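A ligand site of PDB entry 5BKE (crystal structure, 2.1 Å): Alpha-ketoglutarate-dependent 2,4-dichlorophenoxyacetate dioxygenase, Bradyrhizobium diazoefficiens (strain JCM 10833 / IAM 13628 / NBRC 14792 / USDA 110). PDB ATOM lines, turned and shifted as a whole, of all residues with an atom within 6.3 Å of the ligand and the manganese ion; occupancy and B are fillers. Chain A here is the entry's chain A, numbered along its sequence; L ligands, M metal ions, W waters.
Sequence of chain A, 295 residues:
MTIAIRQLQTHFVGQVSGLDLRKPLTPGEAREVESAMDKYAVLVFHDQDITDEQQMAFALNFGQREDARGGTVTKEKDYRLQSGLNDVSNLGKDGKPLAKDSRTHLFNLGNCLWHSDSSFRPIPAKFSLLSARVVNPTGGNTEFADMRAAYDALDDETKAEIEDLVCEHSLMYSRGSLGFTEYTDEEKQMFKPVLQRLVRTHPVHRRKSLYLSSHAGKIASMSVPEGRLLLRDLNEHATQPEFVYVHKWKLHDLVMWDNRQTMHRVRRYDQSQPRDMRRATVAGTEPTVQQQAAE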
ATOM      1  N   VAL A  88      17.570  23.292  -4.518  1.00  0.00           N
ATOM      2  CA  VAL A  88      18.406  24.496  -4.331  1.00  0.00           C
ATOM      3  C   VAL A  88      19.899  24.150  -4.586  1.00  0.00           C
ATOM      4  O   VAL A  88      20.829  24.862  -4.135  1.00  0.00           O
ATOM      5  CB  VAL A  88      18.145  25.190  -2.969  1.00  0.00           C
ATOM      6  CG1 VAL A  88      16.679  25.607  -2.832  1.00  0.00           C
ATOM      7  CG2 VAL A  88      18.521  24.285  -1.815  1.00  0.00           C
ATOM      8  N   ASN A 111      19.711  33.310  -4.063  1.00  0.00           N
ATOM      9  CA  ASN A 111      19.914  32.852  -2.687  1.00  0.00           C
ATOM     10  C   ASN A 111      21.164  33.445  -2.011  1.00  0.00           C
ATOM     11  O   ASN A 111      21.309  33.371  -0.782  1.00  0.00           O
ATOM     12  CB  ASN A 111      19.923  31.325  -2.609  1.00  0.00           C
ATOM     13  CG  ASN A 111      18.563  30.711  -2.949  1.00  0.00           C
ATOM     14  OD1 ASN A 111      17.527  31.382  -2.941  1.00  0.00           O
ATOM     15  ND2 ASN A 111      18.561  29.407  -3.214  1.00  0.00           N
ATOM     16  N   HIS A 115      17.736  36.992   2.462  1.00  0.00           N
ATOM     17  CA  HIS A 115      16.325  36.807   2.162  1.00  0.00           C
ATOM     18  C   HIS A 115      15.637  35.960   3.225  1.00  0.00           C
ATOM     19  O   HIS A 115      16.289  35.270   4.031  1.00  0.00           O
ATOM     20  CB  HIS A 115      16.135  36.207   0.757  1.00  0.00           C
ATOM     21  CG  HIS A 115      16.563  34.767   0.640  1.00  0.00           C
ATOM     22  ND1 HIS A 115      17.870  34.397   0.422  1.00  0.00           N
ATOM     23  CD2 HIS A 115      15.848  33.625   0.736  1.00  0.00           C
ATOM     24  CE1 HIS A 115      17.946  33.072   0.383  1.00  0.00           C
ATOM     25  NE2 HIS A 115      16.723  32.578   0.567  1.00  0.00           N
ATOM     26  N   SER A 116      14.308  36.018   3.199  1.00  0.00           N
ATOM     27  CA  SER A 116      13.460  35.130   3.952  1.00  0.00           C
ATOM     28  C   SER A 116      12.586  34.405   2.931  1.00  0.00           C
ATOM     29  O   SER A 116      12.005  35.042   2.046  1.00  0.00           O
ATOM     30  CB  SER A 116      12.621  35.927   4.940  1.00  0.00           C
ATOM     31  OG  SER A 116      11.811  35.059   5.712  1.00  0.00           O
ATOM     32  N   ASP A 117      12.510  33.076   3.029  1.00  0.00           N
ATOM     33  CA  ASP A 117      11.870  32.267   1.982  1.00  0.00           C
ATOM     34  C   ASP A 117      10.394  32.616   1.738  1.00  0.00           C
ATOM     35  O   ASP A 117       9.654  32.869   2.690  1.00  0.00           O
ATOM     36  CB  ASP A 117      12.014  30.767   2.251  1.00  0.00           C
ATOM     37  CG  ASP A 117      13.460  30.281   2.110  1.00  0.00           C
ATOM     38  OD1 ASP A 117      14.262  30.906   1.394  1.00  0.00           O
ATOM     39  OD2 ASP A 117      13.766  29.251   2.739  1.00  0.00           O
ATOM     40  N   SER A 128      11.775  26.231   6.721  1.00  0.00           N
ATOM     41  CA  SER A 128      12.563  25.623   5.637  1.00  0.00           C
ATOM     42  C   SER A 128      13.603  24.671   6.224  1.00  0.00           C
ATOM     43  O   SER A 128      14.210  24.962   7.251  1.00  0.00           O
ATOM     44  CB  SER A 128      13.249  26.676   4.806  1.00  0.00           C
ATOM     45  OG  SER A 128      12.349  27.581   4.220  1.00  0.00           O
ATOM     46  N   LEU A 130      16.917  22.270   5.163  1.00  0.00           N
ATOM     47  CA  LEU A 130      17.937  22.096   4.142  1.00  0.00           C
ATOM     48  C   LEU A 130      18.919  20.980   4.492  1.00  0.00           C
ATOM     49  O   LEU A 130      19.571  21.015   5.540  1.00  0.00           O
ATOM     50  CB  LEU A 130      18.688  23.409   3.905  1.00  0.00           C
ATOM     51  CG  LEU A 130      19.641  23.510   2.715  1.00  0.00           C
ATOM     52  CD1 LEU A 130      18.902  23.232   1.408  1.00  0.00           C
ATOM     53  CD2 LEU A 130      20.318  24.872   2.668  1.00  0.00           C
ATOM     54  N   GLY A 140      30.356  28.466  -0.062  1.00  0.00           N
ATOM     55  CA  GLY A 140      28.972  28.036   0.107  1.00  0.00           C
ATOM     56  C   GLY A 140      28.541  27.818   1.542  1.00  0.00           C
ATOM     57  O   GLY A 140      27.663  26.991   1.815  1.00  0.00           O
ATOM     58  N   ASN A 141      29.138  28.558   2.480  1.00  0.00           N
ATOM     59  CA  ASN A 141      28.580  28.692   3.828  1.00  0.00           C
ATOM     60  C   ASN A 141      27.162  29.267   3.767  1.00  0.00           C
ATOM     61  O   ASN A 141      26.869  30.106   2.932  1.00  0.00           O
ATOM     62  CB  ASN A 141      29.449  29.626   4.677  1.00  0.00           C
ATOM     63  CG  ASN A 141      30.805  29.029   5.031  1.00  0.00           C
ATOM     64  OD1 ASN A 141      31.079  27.845   4.769  1.00  0.00           O
ATOM     65  ND2 ASN A 141      31.665  29.847   5.635  1.00  0.00           N
ATOM     66  N   THR A 142      26.287  28.802   4.657  1.00  0.00           N
ATOM     67  CA  THR A 142      24.992  29.432   4.790  1.00  0.00           C
ATOM     68  C   THR A 142      24.995  30.270   6.055  1.00  0.00           C
ATOM     69  O   THR A 142      25.317  29.769   7.152  1.00  0.00           O
ATOM     70  CB  THR A 142      23.850  28.409   4.739  1.00  0.00           C
ATOM     71  OG1 THR A 142      23.953  27.692   3.505  1.00  0.00           O
ATOM     72  CG2 THR A 142      22.478  29.083   4.787  1.00  0.00           C
ATOM     73  N   TRP A 249      29.252  23.718   6.290  1.00  0.00           N
ATOM     74  CA  TRP A 249      28.553  22.459   5.993  1.00  0.00           C
ATOM     75  C   TRP A 249      29.428  21.209   6.164  1.00  0.00           C
ATOM     76  O   TRP A 249      30.593  21.188   5.758  1.00  0.00           O
ATOM     77  CB  TRP A 249      27.922  22.493   4.602  1.00  0.00           C
ATOM     78  CG  TRP A 249      26.763  23.457   4.496  1.00  0.00           C
ATOM     79  CD1 TRP A 249      26.808  24.733   4.033  1.00  0.00           C
ATOM     80  CD2 TRP A 249      25.397  23.198   4.859  1.00  0.00           C
ATOM     81  NE1 TRP A 249      25.557  25.305   4.093  1.00  0.00           N
ATOM     82  CE2 TRP A 249      24.673  24.385   4.597  1.00  0.00           C
ATOM     83  CE3 TRP A 249      24.716  22.092   5.388  1.00  0.00           C
ATOM     84  CZ2 TRP A 249      23.293  24.496   4.835  1.00  0.00           C
ATOM     85  CZ3 TRP A 249      23.332  22.204   5.640  1.00  0.00           C
ATOM     86  CH2 TRP A 249      22.645  23.400   5.353  1.00  0.00           C
ATOM     87  N   TRP A 257      15.217  26.330   9.524  1.00  0.00           N
ATOM     88  CA  TRP A 257      15.056  27.694  10.018  1.00  0.00           C
ATOM     89  C   TRP A 257      13.624  28.213   9.954  1.00  0.00           C
ATOM     90  O   TRP A 257      12.840  27.827   9.081  1.00  0.00           O
ATOM     91  CB  TRP A 257      16.028  28.661   9.318  1.00  0.00           C
ATOM     92  CG  TRP A 257      15.830  28.788   7.832  1.00  0.00           C
ATOM     93  CD1 TRP A 257      14.994  29.664   7.186  1.00  0.00           C
ATOM     94  CD2 TRP A 257      16.461  28.016   6.813  1.00  0.00           C
ATOM     95  NE1 TRP A 257      15.072  29.485   5.826  1.00  0.00           N
ATOM     96  CE2 TRP A 257      15.972  28.476   5.568  1.00  0.00           C
ATOM     97  CE3 TRP A 257      17.400  26.966   6.828  1.00  0.00           C
ATOM     98  CZ2 TRP A 257      16.396  27.944   4.328  1.00  0.00           C
ATOM     99  CZ3 TRP A 257      17.829  26.424   5.598  1.00  0.00           C
ATOM    100  CH2 TRP A 257      17.321  26.922   4.360  1.00  0.00           C
ATOM    101  N   ASN A 259      11.585  31.058   8.933  1.00  0.00           N
ATOM    102  CA  ASN A 259      11.624  32.216   8.040  1.00  0.00           C
ATOM    103  C   ASN A 259      10.924  33.413   8.662  1.00  0.00           C
ATOM    104  O   ASN A 259      11.160  34.545   8.257  1.00  0.00           O
ATOM    105  CB  ASN A 259      10.960  31.878   6.699  1.00  0.00           C
ATOM    106  CG  ASN A 259      11.781  30.898   5.887  1.00  0.00           C
ATOM    107  OD1 ASN A 259      12.765  31.285   5.257  1.00  0.00           O
ATOM    108  ND2 ASN A 259      11.380  29.622   5.887  1.00  0.00           N
ATOM    109  N   HIS A 264      18.481  34.521   5.755  1.00  0.00           N
ATOM    110  CA  HIS A 264      19.593  33.623   5.473  1.00  0.00           C
ATOM    111  C   HIS A 264      20.132  33.942   4.100  1.00  0.00           C
ATOM    112  O   HIS A 264      19.458  34.594   3.304  1.00  0.00           O
ATOM    113  CB  HIS A 264      19.153  32.149   5.584  1.00  0.00           C
ATOM    114  CG  HIS A 264      18.056  31.785   4.639  1.00  0.00           C
ATOM    115  ND1 HIS A 264      16.736  32.169   4.845  1.00  0.00           N
ATOM    116  CD2 HIS A 264      18.059  31.096   3.469  1.00  0.00           C
ATOM    117  CE1 HIS A 264      15.995  31.733   3.839  1.00  0.00           C
ATOM    118  NE2 HIS A 264      16.768  31.072   3.003  1.00  0.00           N
ATOM    119  N   ARG A 265      21.356  33.506   3.828  1.00  0.00           N
ATOM    120  CA  ARG A 265      21.975  33.607   2.494  1.00  0.00           C
ATOM    121  C   ARG A 265      23.067  32.564   2.342  1.00  0.00           C
ATOM    122  O   ARG A 265      23.657  32.119   3.338  1.00  0.00           O
ATOM    123  CB  ARG A 265      22.551  35.016   2.228  1.00  0.00           C
ATOM    124  CG  ARG A 265      23.764  35.380   3.068  1.00  0.00           C
ATOM    125  CD  ARG A 265      24.405  36.687   2.633  1.00  0.00           C
ATOM    126  NE  ARG A 265      25.537  37.045   3.499  1.00  0.00           N
ATOM    127  CZ  ARG A 265      26.371  38.063   3.288  1.00  0.00           C
ATOM    128  NH1 ARG A 265      26.234  38.829   2.223  1.00  0.00           N
ATOM    129  NH2 ARG A 265      27.379  38.292   4.133  1.00  0.00           N
ATOM    130  N   VAL A 266      23.329  32.174   1.099  1.00  0.00           N
ATOM    131  CA  VAL A 266      24.468  31.341   0.757  1.00  0.00           C
ATOM    132  C   VAL A 266      25.636  32.223   0.248  1.00  0.00           C
ATOM    133  O   VAL A 266      25.446  33.110  -0.585  1.00  0.00           O
ATOM    134  CB  VAL A 266      24.086  30.194  -0.228  1.00  0.00           C
ATOM    135  CG1 VAL A 266      23.527  30.724  -1.543  1.00  0.00           C
ATOM    136  CG2 VAL A 266      25.252  29.245  -0.470  1.00  0.00           C
ATOM    137  N   ARG A 267      26.837  31.977   0.773  1.00  0.00           N
ATOM    138  CA  ARG A 267      28.056  32.661   0.315  1.00  0.00           C
ATOM    139  C   ARG A 267      28.526  32.048  -1.004  1.00  0.00           C
ATOM    140  O   ARG A 267      28.166  30.917  -1.337  1.00  0.00           O
ATOM    141  CB  ARG A 267      29.164  32.578   1.386  1.00  0.00           C
ATOM    142  CG  ARG A 267      28.855  33.240   2.741  1.00  0.00           C
ATOM    143  CD  ARG A 267      28.106  34.572   2.661  1.00  0.00           C
ATOM    144  NE  ARG A 267      28.855  35.649   1.991  1.00  0.00           N
ATOM    145  CZ  ARG A 267      29.733  36.469   2.579  1.00  0.00           C
ATOM    146  NH1 ARG A 267      30.010  36.352   3.874  1.00  0.00           N
ATOM    147  NH2 ARG A 267      30.337  37.399   1.851  1.00  0.00           N
ATOM    148  N   TYR A 269      30.289  30.210  -4.003  1.00  0.00           N
ATOM    149  CA  TYR A 269      30.911  28.883  -4.090  1.00  0.00           C
ATOM    150  C   TYR A 269      31.413  28.586  -5.504  1.00  0.00           C
ATOM    151  O   TYR A 269      31.037  29.266  -6.459  1.00  0.00           O
ATOM    152  CB  TYR A 269      29.970  27.777  -3.578  1.00  0.00           C
ATOM    153  CG  TYR A 269      28.577  27.789  -4.173  1.00  0.00           C
ATOM    154  CD1 TYR A 269      27.540  28.525  -3.581  1.00  0.00           C
ATOM    155  CD2 TYR A 269      28.275  27.054  -5.329  1.00  0.00           C
ATOM    156  CE1 TYR A 269      26.256  28.543  -4.112  1.00  0.00           C
ATOM    157  CE2 TYR A 269      26.999  27.055  -5.872  1.00  0.00           C
ATOM    158  CZ  TYR A 269      25.994  27.798  -5.262  1.00  0.00           C
ATOM    159  OH  TYR A 269      24.715  27.817  -5.806  1.00  0.00           O
ATOM    160  N   ARG A 275      27.188  20.774  -5.782  1.00  0.00           N
ATOM    161  CA  ARG A 275      26.634  21.209  -4.500  1.00  0.00           C
ATOM    162  C   ARG A 275      25.190  20.722  -4.476  1.00  0.00           C
ATOM    163  O   ARG A 275      24.326  21.369  -5.051  1.00  0.00           O
ATOM    164  CB  ARG A 275      26.678  22.751  -4.368  1.00  0.00           C
ATOM    165  CG  ARG A 275      26.374  23.258  -2.970  1.00  0.00           C
ATOM    166  CD  ARG A 275      26.625  24.755  -2.830  1.00  0.00           C
ATOM    167  NE  ARG A 275      26.491  25.203  -1.436  1.00  0.00           N
ATOM    168  CZ  ARG A 275      25.365  25.645  -0.857  1.00  0.00           C
ATOM    169  NH1 ARG A 275      24.213  25.700  -1.525  1.00  0.00           N
ATOM    170  NH2 ARG A 275      25.389  26.023   0.411  1.00  0.00           N
ATOM    171  N   MET A 277      22.120  20.284  -2.479  1.00  0.00           N
ATOM    172  CA  MET A 277      21.352  20.759  -1.333  1.00  0.00           C
ATOM    173  C   MET A 277      19.867  20.715  -1.696  1.00  0.00           C
ATOM    174  O   MET A 277      19.484  21.128  -2.803  1.00  0.00           O
ATOM    175  CB  MET A 277      21.761  22.184  -0.969  1.00  0.00           C
ATOM    176  CG  MET A 277      23.268  22.418  -0.923  1.00  0.00           C
ATOM    177  SD  MET A 277      24.134  21.587   0.430  1.00  0.00           S
ATOM    178  CE  MET A 277      23.492  22.488   1.844  1.00  0.00           C
ATOM    179  N   ARG A 278      19.059  20.194  -0.777  1.00  0.00           N
ATOM    180  CA  ARG A 278      17.640  19.920  -1.010  1.00  0.00           C
ATOM    181  C   ARG A 278      16.807  20.461   0.151  1.00  0.00           C
ATOM    182  O   ARG A 278      17.111  20.215   1.317  1.00  0.00           O
ATOM    183  CB  ARG A 278      17.392  18.416  -1.171  1.00  0.00           C
ATOM    184  CG  ARG A 278      18.308  17.770  -2.206  1.00  0.00           C
ATOM    185  CD  ARG A 278      17.910  16.361  -2.544  1.00  0.00           C
ATOM    186  NE  ARG A 278      18.982  15.730  -3.298  1.00  0.00           N
ATOM    187  CZ  ARG A 278      18.970  14.484  -3.762  1.00  0.00           C
ATOM    188  NH1 ARG A 278      20.018  14.032  -4.432  1.00  0.00           N
ATOM    189  NH2 ARG A 278      17.935  13.679  -3.546  1.00  0.00           N
ATOM    190  N   ARG A 279      15.770  21.220  -0.200  1.00  0.00           N
ATOM    191  CA  ARG A 279      14.972  21.930   0.781  1.00  0.00           C
ATOM    192  C   ARG A 279      13.557  21.352   0.869  1.00  0.00           C
ATOM    193  O   ARG A 279      12.954  21.005  -0.147  1.00  0.00           O
ATOM    194  CB  ARG A 279      14.941  23.433   0.459  1.00  0.00           C
ATOM    195  CG  ARG A 279      14.436  24.290   1.606  1.00  0.00           C
ATOM    196  CD  ARG A 279      14.287  25.744   1.218  1.00  0.00           C
ATOM    197  NE  ARG A 279      13.039  26.031   0.513  1.00  0.00           N
ATOM    198  CZ  ARG A 279      12.828  27.084  -0.264  1.00  0.00           C
ATOM    199  NH1 ARG A 279      13.789  27.976  -0.483  1.00  0.00           N
ATOM    200  NH2 ARG A 279      11.647  27.251  -0.855  1.00  0.00           N
HETATM  201  C1  LIG L   1      17.193  27.904   0.588  1.00  0.00           C
HETATM  202  C2  LIG L   1      18.438  28.634   0.502  1.00  0.00           C
HETATM  203  C3  LIG L   1      20.838  28.356   0.989  1.00  0.00           C
HETATM  204  C4  LIG L   1      21.937  27.430   0.532  1.00  0.00           C
HETATM  205  O1  LIG L   1      16.119  28.524   0.778  1.00  0.00           O
HETATM  206  O2  LIG L   1      17.266  26.663   0.501  1.00  0.00           O
HETATM  207  O3  LIG L   1      18.390  29.870   0.471  1.00  0.00           O
HETATM  208  O4  LIG L   1      22.868  27.207   1.341  1.00  0.00           O
HETATM  209  N1  LIG L   1      19.559  27.912   0.478  1.00  0.00           N
HETATM  210  O5  LIG L   1      21.903  26.936  -0.633  1.00  0.00           O
HETATM  211 MN    MN M   1      16.357  30.581   0.960  1.00  0.00          MN
HETATM  212  O   HOH W   1      15.796  30.431  -1.118  1.00  0.00           O
HETATM  213  O   HOH W   2      21.119  27.614  -3.181  1.00  0.00           O
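O4 of the ligand sits at hydrogen-bond distance from OG1 of Thr 142 (2.5 Å).
O2 of the ligand is in salt-bridge range of NH1 of Arg 279, 3.8 Å away.
O5 of the ligand lies within salt-bridge range of NH1 of Arg 275, at 2.8 Å.
NH1 of Arg 279 lies within salt-bridge range of OD2 of Asp 117 (3.5 Å).
The side-chain carboxylate of Asp 117 lies close to the indole nitrogen of Trp 257.
N of Asp 117 lies within hydrogen-bond range of OD1 of Asn 259 (2.9 Å).
The side-chain hydroxyl (OG1) of Thr 142 is in hydrogen-bond range of the indole nitrogen (NE1) of Trp 249, 2.9 Å away.
O of Gly 140 lies within hydrogen-bond range of NH2 of Arg 275 (2.8 Å).
N of Val 266 is in hydrogen-bond range of O of Asn 111 (3.0 Å).
The backbone carbonyl oxygen (O) of Met 277 sits at hydrogen-bond distance from the backbone NH (N) of Val 88.
The backbone carbonyl oxygen (O) of Ser 128 sits at hydrogen-bond distance from the backbone NH (N) of Trp 257 (2.8 Å).
CG1 of Val 88 touches O2 of the ligand, at 3.5 Å.
Asn 111 touches the ligand.
Leu 130 touches the ligand (CD2 to O4, 3.7 Å).
Trp 257 touches the ligand (CZ2 to O1, 3.6 Å).
CB of Val 266 touches C4 of the ligand (3.6 Å).
Hydrophobic or aromatic side chains within 4 Å of the ligand: Val 88, His 115, Leu 130, Trp 257, His 264 and Val 266.
Merely in contact with the manganese ion: Arg 279.
Four residues have an atom within 4 Å of the manganese ion: His 115, Asp 117, His 264 and Arg 279.
The nearest printed residue that does not touch the manganese ion is Asn 111 (4.2 Å).
The manganese ion is bound by NE2 of His 115 (2.1 Å), O1 of the ligand (2.1 Å), NE2 of His 264 (2.1 Å), water W1 (2.2 Å), OD1 of Asp 117 (2.2 Å) and O3 of the ligand (2.2 Å).
The manganese ion has six donor atoms within binding distance.
Water W1 bridges OD1 of Asn 111 (2.7 Å) and NH1 of Arg 279 (3.2 Å).
Water W2 lies within hydrogen-bond range of O5 of the ligand (2.8 Å), O of Val 88 (2.9 Å) and ND2 of Asn 111 (3.1 Å).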
